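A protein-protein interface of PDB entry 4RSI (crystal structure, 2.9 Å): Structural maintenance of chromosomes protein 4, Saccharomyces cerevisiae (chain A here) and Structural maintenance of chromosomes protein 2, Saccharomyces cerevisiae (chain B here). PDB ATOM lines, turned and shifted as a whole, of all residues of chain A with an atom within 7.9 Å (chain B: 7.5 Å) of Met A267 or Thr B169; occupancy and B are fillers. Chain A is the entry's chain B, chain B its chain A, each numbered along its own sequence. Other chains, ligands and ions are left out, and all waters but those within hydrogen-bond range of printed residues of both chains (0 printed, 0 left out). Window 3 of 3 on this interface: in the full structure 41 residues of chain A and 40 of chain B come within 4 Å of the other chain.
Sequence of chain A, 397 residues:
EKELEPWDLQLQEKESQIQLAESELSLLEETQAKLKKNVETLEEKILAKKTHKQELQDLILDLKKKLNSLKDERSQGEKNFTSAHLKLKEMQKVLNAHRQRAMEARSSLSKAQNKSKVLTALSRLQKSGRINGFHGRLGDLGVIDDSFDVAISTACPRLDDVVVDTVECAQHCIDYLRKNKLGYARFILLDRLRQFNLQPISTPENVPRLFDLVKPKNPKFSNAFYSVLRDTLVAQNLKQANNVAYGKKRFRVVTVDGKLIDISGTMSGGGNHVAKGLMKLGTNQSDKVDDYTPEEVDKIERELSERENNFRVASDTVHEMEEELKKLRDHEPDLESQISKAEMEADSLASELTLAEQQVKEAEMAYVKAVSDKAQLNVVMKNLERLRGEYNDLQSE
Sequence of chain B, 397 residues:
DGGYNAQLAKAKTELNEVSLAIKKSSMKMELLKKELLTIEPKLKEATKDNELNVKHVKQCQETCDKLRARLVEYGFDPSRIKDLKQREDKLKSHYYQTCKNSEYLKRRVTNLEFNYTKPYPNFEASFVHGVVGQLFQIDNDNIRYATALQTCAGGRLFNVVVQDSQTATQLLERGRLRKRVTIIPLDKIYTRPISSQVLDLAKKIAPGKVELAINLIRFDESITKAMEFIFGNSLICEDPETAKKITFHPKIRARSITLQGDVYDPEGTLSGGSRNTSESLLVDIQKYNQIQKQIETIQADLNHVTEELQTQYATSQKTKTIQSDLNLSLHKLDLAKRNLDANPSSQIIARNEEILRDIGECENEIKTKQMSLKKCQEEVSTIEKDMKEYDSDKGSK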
ATOM      1  N   LEU A 238      25.591  -3.730  -7.576  1.00  0.00           N
ATOM      2  CA  LEU A 238      24.590  -2.736  -7.174  1.00  0.00           C
ATOM      3  C   LEU A 238      24.554  -2.352  -5.675  1.00  0.00           C
ATOM      4  O   LEU A 238      23.478  -2.268  -5.061  1.00  0.00           O
ATOM      5  CB  LEU A 238      23.199  -3.165  -7.679  1.00  0.00           C
ATOM      6  CG  LEU A 238      23.125  -3.539  -9.169  1.00  0.00           C
ATOM      7  CD1 LEU A 238      21.932  -4.483  -9.444  1.00  0.00           C
ATOM      8  CD2 LEU A 238      23.055  -2.287 -10.052  1.00  0.00           C
ATOM      9  N   GLN A 240      25.932   0.358  -5.633  1.00  0.00           N
ATOM     10  CA  GLN A 240      25.993   1.672  -6.263  1.00  0.00           C
ATOM     11  C   GLN A 240      24.764   2.573  -6.027  1.00  0.00           C
ATOM     12  O   GLN A 240      24.905   3.672  -5.508  1.00  0.00           O
ATOM     13  CB  GLN A 240      26.270   1.516  -7.744  1.00  0.00           C
ATOM     14  N   ALA A 241      23.564   2.125  -6.390  1.00  0.00           N
ATOM     15  CA  ALA A 241      22.374   2.980  -6.258  1.00  0.00           C
ATOM     16  C   ALA A 241      22.180   3.590  -4.859  1.00  0.00           C
ATOM     17  O   ALA A 241      21.412   4.537  -4.687  1.00  0.00           O
ATOM     18  CB  ALA A 241      21.112   2.232  -6.709  1.00  0.00           C
ATOM     19  N   ALA A 245      23.920   7.496  -6.044  1.00  0.00           N
ATOM     20  CA  ALA A 245      22.735   8.355  -6.136  1.00  0.00           C
ATOM     21  C   ALA A 245      22.658   9.387  -5.020  1.00  0.00           C
ATOM     22  O   ALA A 245      22.223  10.520  -5.235  1.00  0.00           O
ATOM     23  CB  ALA A 245      21.471   7.513  -6.154  1.00  0.00           C
ATOM     24  N   LYS A 259      27.825  -2.040 -15.032  1.00  0.00           N
ATOM     25  CA  LYS A 259      26.777  -1.021 -15.046  1.00  0.00           C
ATOM     26  C   LYS A 259      27.333   0.351 -14.622  1.00  0.00           C
ATOM     27  O   LYS A 259      28.427   0.435 -14.042  1.00  0.00           O
ATOM     28  CB  LYS A 259      25.554  -1.441 -14.216  1.00  0.00           C
ATOM     29  CG  LYS A 259      24.851  -2.691 -14.742  1.00  0.00           C
ATOM     30  CD  LYS A 259      23.654  -3.075 -13.872  1.00  0.00           C
ATOM     31  CE  LYS A 259      23.355  -4.584 -13.907  1.00  0.00           C
ATOM     32  NZ  LYS A 259      24.091  -5.364 -12.851  1.00  0.00           N
ATOM     33  N   LEU A 260      26.597   1.422 -14.939  1.00  0.00           N
ATOM     34  CA  LEU A 260      27.077   2.785 -14.688  1.00  0.00           C
ATOM     35  C   LEU A 260      26.015   3.780 -14.191  1.00  0.00           C
ATOM     36  O   LEU A 260      24.995   4.009 -14.845  1.00  0.00           O
ATOM     37  CB  LEU A 260      27.761   3.351 -15.938  1.00  0.00           C
ATOM     38  CG  LEU A 260      29.007   4.196 -15.667  1.00  0.00           C
ATOM     39  CD1 LEU A 260      29.817   4.425 -16.935  1.00  0.00           C
ATOM     40  CD2 LEU A 260      28.653   5.520 -14.988  1.00  0.00           C
ATOM     41  N   ILE A 261      26.278   4.382 -13.033  1.00  0.00           N
ATOM     42  CA  ILE A 261      25.524   5.543 -12.598  1.00  0.00           C
ATOM     43  C   ILE A 261      26.473   6.729 -12.554  1.00  0.00           C
ATOM     44  O   ILE A 261      27.429   6.719 -11.785  1.00  0.00           O
ATOM     45  CB  ILE A 261      24.904   5.345 -11.215  1.00  0.00           C
ATOM     46  CG1 ILE A 261      24.136   4.019 -11.172  1.00  0.00           C
ATOM     47  CG2 ILE A 261      23.983   6.522 -10.862  1.00  0.00           C
ATOM     48  CD1 ILE A 261      23.224   3.866  -9.968  1.00  0.00           C
ATOM     49  N   ASP A 262      26.206   7.738 -13.385  1.00  0.00           N
ATOM     50  CA  ASP A 262      27.048   8.926 -13.496  1.00  0.00           C
ATOM     51  C   ASP A 262      26.640   9.988 -12.483  1.00  0.00           C
ATOM     52  O   ASP A 262      25.634   9.842 -11.795  1.00  0.00           O
ATOM     53  CB  ASP A 262      26.961   9.493 -14.905  1.00  0.00           C
ATOM     54  CG  ASP A 262      28.089  10.457 -15.215  1.00  0.00           C
ATOM     55  OD1 ASP A 262      28.312  11.403 -14.416  1.00  0.00           O
ATOM     56  OD2 ASP A 262      28.757  10.261 -16.260  1.00  0.00           O
ATOM     57  N   ILE A 263      27.431  11.053 -12.386  1.00  0.00           N
ATOM     58  CA  ILE A 263      27.174  12.085 -11.394  1.00  0.00           C
ATOM     59  C   ILE A 263      25.837  12.714 -11.706  1.00  0.00           C
ATOM     60  O   ILE A 263      25.076  13.066 -10.814  1.00  0.00           O
ATOM     61  CB  ILE A 263      28.244  13.185 -11.420  1.00  0.00           C
ATOM     62  CG1 ILE A 263      29.635  12.586 -11.627  1.00  0.00           C
ATOM     63  CG2 ILE A 263      28.202  13.993 -10.114  1.00  0.00           C
ATOM     64  CD1 ILE A 263      30.317  12.166 -10.333  1.00  0.00           C
ATOM     65  N   SER A 264      25.565  12.824 -12.995  1.00  0.00           N
ATOM     66  CA  SER A 264      24.372  13.481 -13.508  1.00  0.00           C
ATOM     67  C   SER A 264      23.050  12.935 -12.977  1.00  0.00           C
ATOM     68  O   SER A 264      22.089  13.683 -12.829  1.00  0.00           O
ATOM     69  CB  SER A 264      24.380  13.397 -15.036  1.00  0.00           C
ATOM     70  OG  SER A 264      24.987  12.191 -15.480  1.00  0.00           O
ATOM     71  N   GLY A 265      23.012  11.636 -12.697  1.00  0.00           N
ATOM     72  CA  GLY A 265      21.754  10.949 -12.468  1.00  0.00           C
ATOM     73  C   GLY A 265      21.565   9.844 -13.508  1.00  0.00           C
ATOM     74  O   GLY A 265      20.765   8.934 -13.305  1.00  0.00           O
ATOM     75  N   THR A 266      22.295   9.945 -14.624  1.00  0.00           N
ATOM     76  CA  THR A 266      22.398   8.884 -15.624  1.00  0.00           C
ATOM     77  C   THR A 266      22.466   7.526 -14.922  1.00  0.00           C
ATOM     78  O   THR A 266      23.080   7.409 -13.862  1.00  0.00           O
ATOM     79  CB  THR A 266      23.683   9.062 -16.473  1.00  0.00           C
ATOM     80  OG1 THR A 266      23.396   9.841 -17.642  1.00  0.00           O
ATOM     81  CG2 THR A 266      24.294   7.700 -16.883  1.00  0.00           C
ATOM     82  N   MET A 267      21.804   6.515 -15.488  1.00  0.00           N
ATOM     83  CA  MET A 267      21.861   5.142 -14.980  1.00  0.00           C
ATOM     84  C   MET A 267      21.928   4.199 -16.191  1.00  0.00           C
ATOM     85  O   MET A 267      20.924   3.958 -16.888  1.00  0.00           O
ATOM     86  CB  MET A 267      20.637   4.833 -14.102  1.00  0.00           C
ATOM     87  CG  MET A 267      20.863   3.719 -13.037  1.00  0.00           C
ATOM     88  SD  MET A 267      19.315   3.027 -12.356  1.00  0.00           S
ATOM     89  CE  MET A 267      18.630   4.445 -11.444  1.00  0.00           C
ATOM     90  N   SER A 268      23.120   3.685 -16.456  1.00  0.00           N
ATOM     91  CA  SER A 268      23.350   2.953 -17.690  1.00  0.00           C
ATOM     92  C   SER A 268      23.577   1.468 -17.451  1.00  0.00           C
ATOM     93  O   SER A 268      24.582   1.071 -16.854  1.00  0.00           O
ATOM     94  CB  SER A 268      24.530   3.558 -18.455  1.00  0.00           C
ATOM     95  OG  SER A 268      25.139   2.600 -19.310  1.00  0.00           O
ATOM     96  N   GLY A 269      22.638   0.655 -17.941  1.00  0.00           N
ATOM     97  CA  GLY A 269      22.697  -0.790 -17.807  1.00  0.00           C
ATOM     98  C   GLY A 269      22.562  -1.528 -19.129  1.00  0.00           C
ATOM     99  O   GLY A 269      21.719  -1.188 -19.961  1.00  0.00           O
ATOM    100  N   GLY A 270      23.386  -2.562 -19.303  1.00  0.00           N
ATOM    101  CA  GLY A 270      23.498  -3.277 -20.561  1.00  0.00           C
ATOM    102  C   GLY A 270      22.423  -4.305 -20.866  1.00  0.00           C
ATOM    103  O   GLY A 270      21.280  -4.269 -20.361  1.00  0.00           O
ATOM    104  N   PRO B 119       7.742  -4.560 -16.374  1.00  0.00           N
ATOM    105  CA  PRO B 119       8.380  -5.225 -15.228  1.00  0.00           C
ATOM    106  C   PRO B 119       7.377  -5.830 -14.223  1.00  0.00           C
ATOM    107  O   PRO B 119       7.627  -6.911 -13.673  1.00  0.00           O
ATOM    108  CB  PRO B 119       9.199  -4.092 -14.577  1.00  0.00           C
ATOM    109  CG  PRO B 119       9.287  -2.985 -15.636  1.00  0.00           C
ATOM    110  CD  PRO B 119       8.009  -3.113 -16.422  1.00  0.00           C
ATOM    111  N   VAL B 160      17.110   6.932 -22.980  1.00  0.00           N
ATOM    112  CA  VAL B 160      15.682   6.887 -22.666  1.00  0.00           C
ATOM    113  C   VAL B 160      15.314   7.821 -21.526  1.00  0.00           C
ATOM    114  O   VAL B 160      15.984   7.863 -20.518  1.00  0.00           O
ATOM    115  CB  VAL B 160      15.209   5.478 -22.284  1.00  0.00           C
ATOM    116  CG1 VAL B 160      13.765   5.526 -21.771  1.00  0.00           C
ATOM    117  CG2 VAL B 160      15.367   4.501 -23.458  1.00  0.00           C
ATOM    118  N   VAL B 162      12.919   8.633 -18.528  1.00  0.00           N
ATOM    119  CA  VAL B 162      11.912   8.055 -17.609  1.00  0.00           C
ATOM    120  C   VAL B 162      11.473   9.002 -16.483  1.00  0.00           C
ATOM    121  O   VAL B 162      12.163   9.971 -16.145  1.00  0.00           O
ATOM    122  CB  VAL B 162      12.403   6.765 -16.968  1.00  0.00           C
ATOM    123  CG1 VAL B 162      13.054   5.910 -17.997  1.00  0.00           C
ATOM    124  CG2 VAL B 162      13.395   7.086 -15.875  1.00  0.00           C
ATOM    125  N   ASP B 164      11.208   8.687 -13.148  1.00  0.00           N
ATOM    126  CA  ASP B 164      11.972   8.757 -11.897  1.00  0.00           C
ATOM    127  C   ASP B 164      12.946   7.601 -11.732  1.00  0.00           C
ATOM    128  O   ASP B 164      12.767   6.512 -12.309  1.00  0.00           O
ATOM    129  CB  ASP B 164      11.053   8.852 -10.669  1.00  0.00           C
ATOM    130  CG  ASP B 164       9.983   7.786 -10.668  1.00  0.00           C
ATOM    131  OD1 ASP B 164      10.361   6.593 -10.590  1.00  0.00           O
ATOM    132  OD2 ASP B 164       8.778   8.143 -10.762  1.00  0.00           O
ATOM    133  N   SER B 165      13.972   7.855 -10.926  1.00  0.00           N
ATOM    134  CA  SER B 165      15.124   6.973 -10.824  1.00  0.00           C
ATOM    135  C   SER B 165      14.761   5.521 -10.584  1.00  0.00           C
ATOM    136  O   SER B 165      15.517   4.620 -10.966  1.00  0.00           O
ATOM    137  CB  SER B 165      16.036   7.437  -9.707  1.00  0.00           C
ATOM    138  OG  SER B 165      17.241   6.704  -9.752  1.00  0.00           O
ATOM    139  N   GLN B 166      13.615   5.305  -9.939  1.00  0.00           N
ATOM    140  CA  GLN B 166      13.157   3.955  -9.630  1.00  0.00           C
ATOM    141  C   GLN B 166      12.799   3.233 -10.917  1.00  0.00           C
ATOM    142  O   GLN B 166      13.248   2.099 -11.170  1.00  0.00           O
ATOM    143  CB  GLN B 166      11.965   3.998  -8.680  1.00  0.00           C
ATOM    144  N   THR B 167      11.997   3.913 -11.731  1.00  0.00           N
ATOM    145  CA  THR B 167      11.547   3.360 -12.997  1.00  0.00           C
ATOM    146  C   THR B 167      12.761   2.951 -13.843  1.00  0.00           C
ATOM    147  O   THR B 167      12.735   1.969 -14.561  1.00  0.00           O
ATOM    148  CB  THR B 167      10.663   4.365 -13.753  1.00  0.00           C
ATOM    149  OG1 THR B 167       9.709   4.951 -12.855  1.00  0.00           O
ATOM    150  CG2 THR B 167       9.937   3.685 -14.878  1.00  0.00           C
ATOM    151  N   ALA B 168      13.839   3.704 -13.727  1.00  0.00           N
ATOM    152  CA  ALA B 168      15.071   3.362 -14.419  1.00  0.00           C
ATOM    153  C   ALA B 168      15.624   2.020 -13.959  1.00  0.00           C
ATOM    154  O   ALA B 168      15.934   1.146 -14.781  1.00  0.00           O
ATOM    155  CB  ALA B 168      16.087   4.452 -14.202  1.00  0.00           C
ATOM    156  N   THR B 169      15.735   1.876 -12.639  1.00  0.00           N
ATOM    157  CA  THR B 169      16.277   0.672 -12.000  1.00  0.00           C
ATOM    158  C   THR B 169      15.436  -0.547 -12.305  1.00  0.00           C
ATOM    159  O   THR B 169      15.968  -1.632 -12.547  1.00  0.00           O
ATOM    160  CB  THR B 169      16.352   0.819 -10.477  1.00  0.00           C
ATOM    161  OG1 THR B 169      15.912   2.135 -10.099  1.00  0.00           O
ATOM    162  CG2 THR B 169      17.794   0.549  -9.971  1.00  0.00           C
ATOM    163  N   GLN B 170      14.121  -0.366 -12.293  1.00  0.00           N
ATOM    164  CA  GLN B 170      13.239  -1.444 -12.710  1.00  0.00           C
ATOM    165  C   GLN B 170      13.530  -1.877 -14.153  1.00  0.00           C
ATOM    166  O   GLN B 170      13.700  -3.071 -14.430  1.00  0.00           O
ATOM    167  CB  GLN B 170      11.778  -1.035 -12.575  1.00  0.00           C
ATOM    168  CG  GLN B 170      11.349  -0.783 -11.160  1.00  0.00           C
ATOM    169  CD  GLN B 170       9.885  -0.406 -11.075  1.00  0.00           C
ATOM    170  OE1 GLN B 170       9.521   0.781 -11.138  1.00  0.00           O
ATOM    171  NE2 GLN B 170       9.027  -1.416 -10.948  1.00  0.00           N
ATOM    172  N   LEU B 171      13.587  -0.901 -15.061  1.00  0.00           N
ATOM    173  CA  LEU B 171      13.789  -1.194 -16.469  1.00  0.00           C
ATOM    174  C   LEU B 171      15.084  -1.966 -16.629  1.00  0.00           C
ATOM    175  O   LEU B 171      15.120  -3.033 -17.254  1.00  0.00           O
ATOM    176  CB  LEU B 171      13.799   0.087 -17.303  1.00  0.00           C
ATOM    177  CG  LEU B 171      12.466   0.839 -17.405  1.00  0.00           C
ATOM    178  CD1 LEU B 171      12.664   2.165 -18.115  1.00  0.00           C
ATOM    179  CD2 LEU B 171      11.394   0.016 -18.095  1.00  0.00           C
ATOM    180  N   LEU B 172      16.137  -1.451 -16.014  1.00  0.00           N
ATOM    181  CA  LEU B 172      17.421  -2.120 -16.081  1.00  0.00           C
ATOM    182  C   LEU B 172      17.355  -3.594 -15.692  1.00  0.00           C
ATOM    183  O   LEU B 172      17.769  -4.443 -16.483  1.00  0.00           O
ATOM    184  CB  LEU B 172      18.442  -1.376 -15.238  1.00  0.00           C
ATOM    185  CG  LEU B 172      18.695   0.005 -15.810  1.00  0.00           C
ATOM    186  CD1 LEU B 172      19.546   0.827 -14.850  1.00  0.00           C
ATOM    187  CD2 LEU B 172      19.350  -0.123 -17.194  1.00  0.00           C
ATOM    188  N   GLU B 173      16.809  -3.905 -14.511  1.00  0.00           N
ATOM    189  CA  GLU B 173      16.850  -5.291 -14.003  1.00  0.00           C
ATOM    190  C   GLU B 173      15.697  -6.201 -14.494  1.00  0.00           C
ATOM    191  O   GLU B 173      15.927  -7.190 -15.209  1.00  0.00           O
ATOM    192  CB  GLU B 173      17.004  -5.321 -12.471  1.00  0.00           C
ATOM    193  CG  GLU B 173      15.966  -4.487 -11.679  1.00  0.00           C
ATOM    194  CD  GLU B 173      16.327  -4.274 -10.187  1.00  0.00           C
ATOM    195  OE1 GLU B 173      15.398  -3.960  -9.399  1.00  0.00           O
ATOM    196  OE2 GLU B 173      17.525  -4.396  -9.806  1.00  0.00           O
ATOM    197  N   ARG B 174      14.464  -5.849 -14.141  1.00  0.00           N
ATOM    198  CA  ARG B 174      13.310  -6.670 -14.486  1.00  0.00           C
ATOM    199  C   ARG B 174      12.602  -6.204 -15.754  1.00  0.00           C
ATOM    200  O   ARG B 174      11.380  -6.037 -15.759  1.00  0.00           O
ATOM    201  CB  ARG B 174      12.312  -6.714 -13.320  1.00  0.00           C
ATOM    202  CG  ARG B 174      11.750  -8.120 -13.044  1.00  0.00           C
ATOM    203  CD  ARG B 174      10.751  -8.159 -11.876  1.00  0.00           C
ATOM    204  NE  ARG B 174      11.298  -7.591 -10.645  1.00  0.00           N
ATOM    205  CZ  ARG B 174      12.163  -8.214  -9.850  1.00  0.00           C
ATOM    206  NH1 ARG B 174      12.594  -9.435 -10.156  1.00  0.00           N
ATOM    207  NH2 ARG B 174      12.609  -7.613  -8.753  1.00  0.00           N
ATOM    208  N   GLY B 175      13.347  -6.016 -16.838  1.00  0.00           N
ATOM    209  CA  GLY B 175      12.749  -5.456 -18.041  1.00  0.00           C
ATOM    210  C   GLY B 175      13.267  -6.108 -19.294  1.00  0.00           C
ATOM    211  O   GLY B 175      12.751  -5.863 -20.386  1.00  0.00           O
ATOM    212  N   ARG B 180      22.314  -2.745 -24.370  1.00  0.00           N
ATOM    213  CA  ARG B 180      22.668  -1.686 -23.417  1.00  0.00           C
ATOM    214  C   ARG B 180      21.974  -0.348 -23.622  1.00  0.00           C
ATOM    215  O   ARG B 180      22.083   0.233 -24.689  1.00  0.00           O
ATOM    216  CB  ARG B 180      24.182  -1.459 -23.499  1.00  0.00           C
ATOM    217  CG  ARG B 180      24.757  -0.485 -22.458  1.00  0.00           C
ATOM    218  CD  ARG B 180      26.211  -0.847 -22.132  1.00  0.00           C
ATOM    219  NE  ARG B 180      26.835   0.061 -21.169  1.00  0.00           N
ATOM    220  CZ  ARG B 180      26.632   0.018 -19.855  1.00  0.00           C
ATOM    221  NH1 ARG B 180      25.809  -0.887 -19.331  1.00  0.00           N
ATOM    222  NH2 ARG B 180      27.245   0.883 -19.059  1.00  0.00           N
ATOM    223  N   VAL B 181      21.296   0.169 -22.607  1.00  0.00           N
ATOM    224  CA  VAL B 181      20.713   1.520 -22.728  1.00  0.00           C
ATOM    225  C   VAL B 181      21.049   2.520 -21.576  1.00  0.00           C
ATOM    226  O   VAL B 181      21.058   2.145 -20.411  1.00  0.00           O
ATOM    227  CB  VAL B 181      19.182   1.449 -22.967  1.00  0.00           C
ATOM    228  CG1 VAL B 181      18.460   1.108 -21.698  1.00  0.00           C
ATOM    229  CG2 VAL B 181      18.656   2.761 -23.471  1.00  0.00           C
ATOM    230  N   THR B 182      21.327   3.783 -21.900  1.00  0.00           N
ATOM    231  CA  THR B 182      21.515   4.813 -20.864  1.00  0.00           C
ATOM    232  C   THR B 182      20.170   5.523 -20.532  1.00  0.00           C
ATOM    233  O   THR B 182      19.374   5.817 -21.421  1.00  0.00           O
ATOM    234  CB  THR B 182      22.645   5.833 -21.244  1.00  0.00           C
ATOM    235  OG1 THR B 182      23.768   5.135 -21.802  1.00  0.00           O
ATOM    236  CG2 THR B 182      23.132   6.635 -20.013  1.00  0.00           C
ATOM    237  N   ILE B 183      19.890   5.774 -19.257  1.00  0.00           N
ATOM    238  CA  ILE B 183      18.535   6.198 -18.902  1.00  0.00           C
ATOM    239  C   ILE B 183      18.563   7.438 -18.057  1.00  0.00           C
ATOM    240  O   ILE B 183      19.096   7.434 -16.957  1.00  0.00           O
ATOM    241  CB  ILE B 183      17.748   5.078 -18.150  1.00  0.00           C
ATOM    242  CG1 ILE B 183      17.526   3.871 -19.058  1.00  0.00           C
ATOM    243  CG2 ILE B 183      16.377   5.568 -17.627  1.00  0.00           C
ATOM    244  CD1 ILE B 183      16.628   2.848 -18.449  1.00  0.00           C
ATOM    245  N   ILE B 184      17.964   8.499 -18.570  1.00  0.00           N
ATOM    246  CA  ILE B 184      18.015   9.811 -17.917  1.00  0.00           C
ATOM    247  C   ILE B 184      16.798   9.909 -17.046  1.00  0.00           C
ATOM    248  O   ILE B 184      15.694   9.971 -17.554  1.00  0.00           O
ATOM    249  CB  ILE B 184      17.984  10.966 -18.977  1.00  0.00           C
ATOM    250  CG1 ILE B 184      19.231  10.942 -19.876  1.00  0.00           C
ATOM    251  CG2 ILE B 184      17.799  12.338 -18.334  1.00  0.00           C
ATOM    252  CD1 ILE B 184      19.018  11.664 -21.154  1.00  0.00           C
ATOM    253  N   PRO B 185      16.983   9.886 -15.731  1.00  0.00           N
ATOM    254  CA  PRO B 185      15.842   9.894 -14.812  1.00  0.00           C
ATOM    255  C   PRO B 185      15.407  11.292 -14.437  1.00  0.00           C
ATOM    256  O   PRO B 185      16.076  11.959 -13.652  1.00  0.00           O
ATOM    257  CB  PRO B 185      16.400   9.177 -13.579  1.00  0.00           C
ATOM    258  CG  PRO B 185      17.686   8.521 -14.054  1.00  0.00           C
ATOM    259  CD  PRO B 185      18.211   9.470 -15.048  1.00  0.00           C
ATOM    260  N   LYS B 188      16.301  13.123 -10.981  1.00  0.00           N
ATOM    261  CA  LYS B 188      17.625  12.977 -10.379  1.00  0.00           C
ATOM    262  C   LYS B 188      18.693  13.793 -11.128  1.00  0.00           C
ATOM    263  O   LYS B 188      19.715  14.158 -10.537  1.00  0.00           O
ATOM    264  CB  LYS B 188      18.037  11.495 -10.309  1.00  0.00           C
ATOM    265  CG  LYS B 188      17.897  10.847  -8.927  1.00  0.00           C
ATOM    266  CD  LYS B 188      18.611   9.471  -8.856  1.00  0.00           C
ATOM    267  CE  LYS B 188      20.153   9.539  -8.896  1.00  0.00           C
ATOM    268  NZ  LYS B 188      20.809   8.197  -9.134  1.00  0.00           N
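The backbone NH of Val B160 is in hydrogen-bond range of the backbone carbonyl oxygen of Thr B182 (3.0 Å). O of Leu A260 is in hydrogen-bond range of N of Ser A268, at 2.5 Å. O of Gln B166 lies within hydrogen-bond range of OG1 of Thr B169 (2.9 Å). The backbone NH of Ser A264 sits close to the side-chain carboxylate of Asp A262 (3.4 Å). The backbone carbonyl oxygen (O) of Ser B165 sits at hydrogen-bond distance from the side-chain hydroxyl (OG1) of Thr B169 (2.7 Å).
Met A267 touches just these residues of chain B: Ser B165 (3.1 Å), Ala B168 (3.8 Å), Thr B169 (3.8 Å), Leu B172 (3.3 Å), Val B181 (3.96 Å) and Ile B183 (3.2 Å). Of chain A, only Met A267 (3.8 Å) comes within 4 Å of Thr B169. Of the printed residues of chain A, Ala B168 touches Met A267 (3.8 Å). Of the printed residues of chain B, Gly A270 touches Arg B180. Of the printed residues of chain A, Ser B165 touches Met A267 (3.1 Å). Arg B174 touches none of the printed residues of chain A. Pro B119 touches none of the printed residues of chain A. The nearest residue of chain B that does not touch Met A267 is Thr B182 (4.04 Å). The nearest residue of chain A that does not touch Thr B169 is Ala A241 (4.9 Å). The nearest printed residue of chain A that does not touch Ile B183 is Gly A265 (4.3 Å).
Of the 16 printed residues of chain A, 9 touch a printed residue of chain B. Hydrophobic or aromatic side chains of chain A within 4 Å of the printed part of chain B: Ala A245, Ile A261 and Met A267. Among the printed residues, 19 pairs touch across the chains. Among the printed residues, no Asp or Glu carboxylate lies within 4 Å of a Lys or Arg side-chain nitrogen of the other chain.
N of Ile B183 lies within hydrogen-bond range of O of Met A267, at 3.2 Å. N of Val B181 sits at hydrogen-bond distance from O of Gly A269 (3.0 Å). The backbone NH (N) of Thr B169 lies close to the side-chain sulfur (SD) of Met A267, at 3.8 Å. The backbone NH (N) of Gly A270 sits close to the guanidinium group (NH1) of Arg B180, at 2.9 Å. The guanidinium group of Arg B180 lies within hydrogen-bond range of the side-chain hydroxyl of Ser A268 (2.7 Å). The backbone carbonyl oxygen of Ser A264 sits close to the backbone carbonyl oxygen of Lys B188 (3.3 Å).
Among the printed residues, merely in contact across the chains: Ala A245 with Lys B188, Gly A265 with Pro B185, Met A267 with Ser B165, Gly A269 with Arg B180, Met A267 with Leu B172, Gly A269 with Leu B172, Thr A266 with Thr B182, Ser A268 with Val B181, Ser A268 with Thr B182, Met A267 with Ala B168, Thr A266 with Ile B183, Met A267 with Val B181 and Ile A261 with Lys B188.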
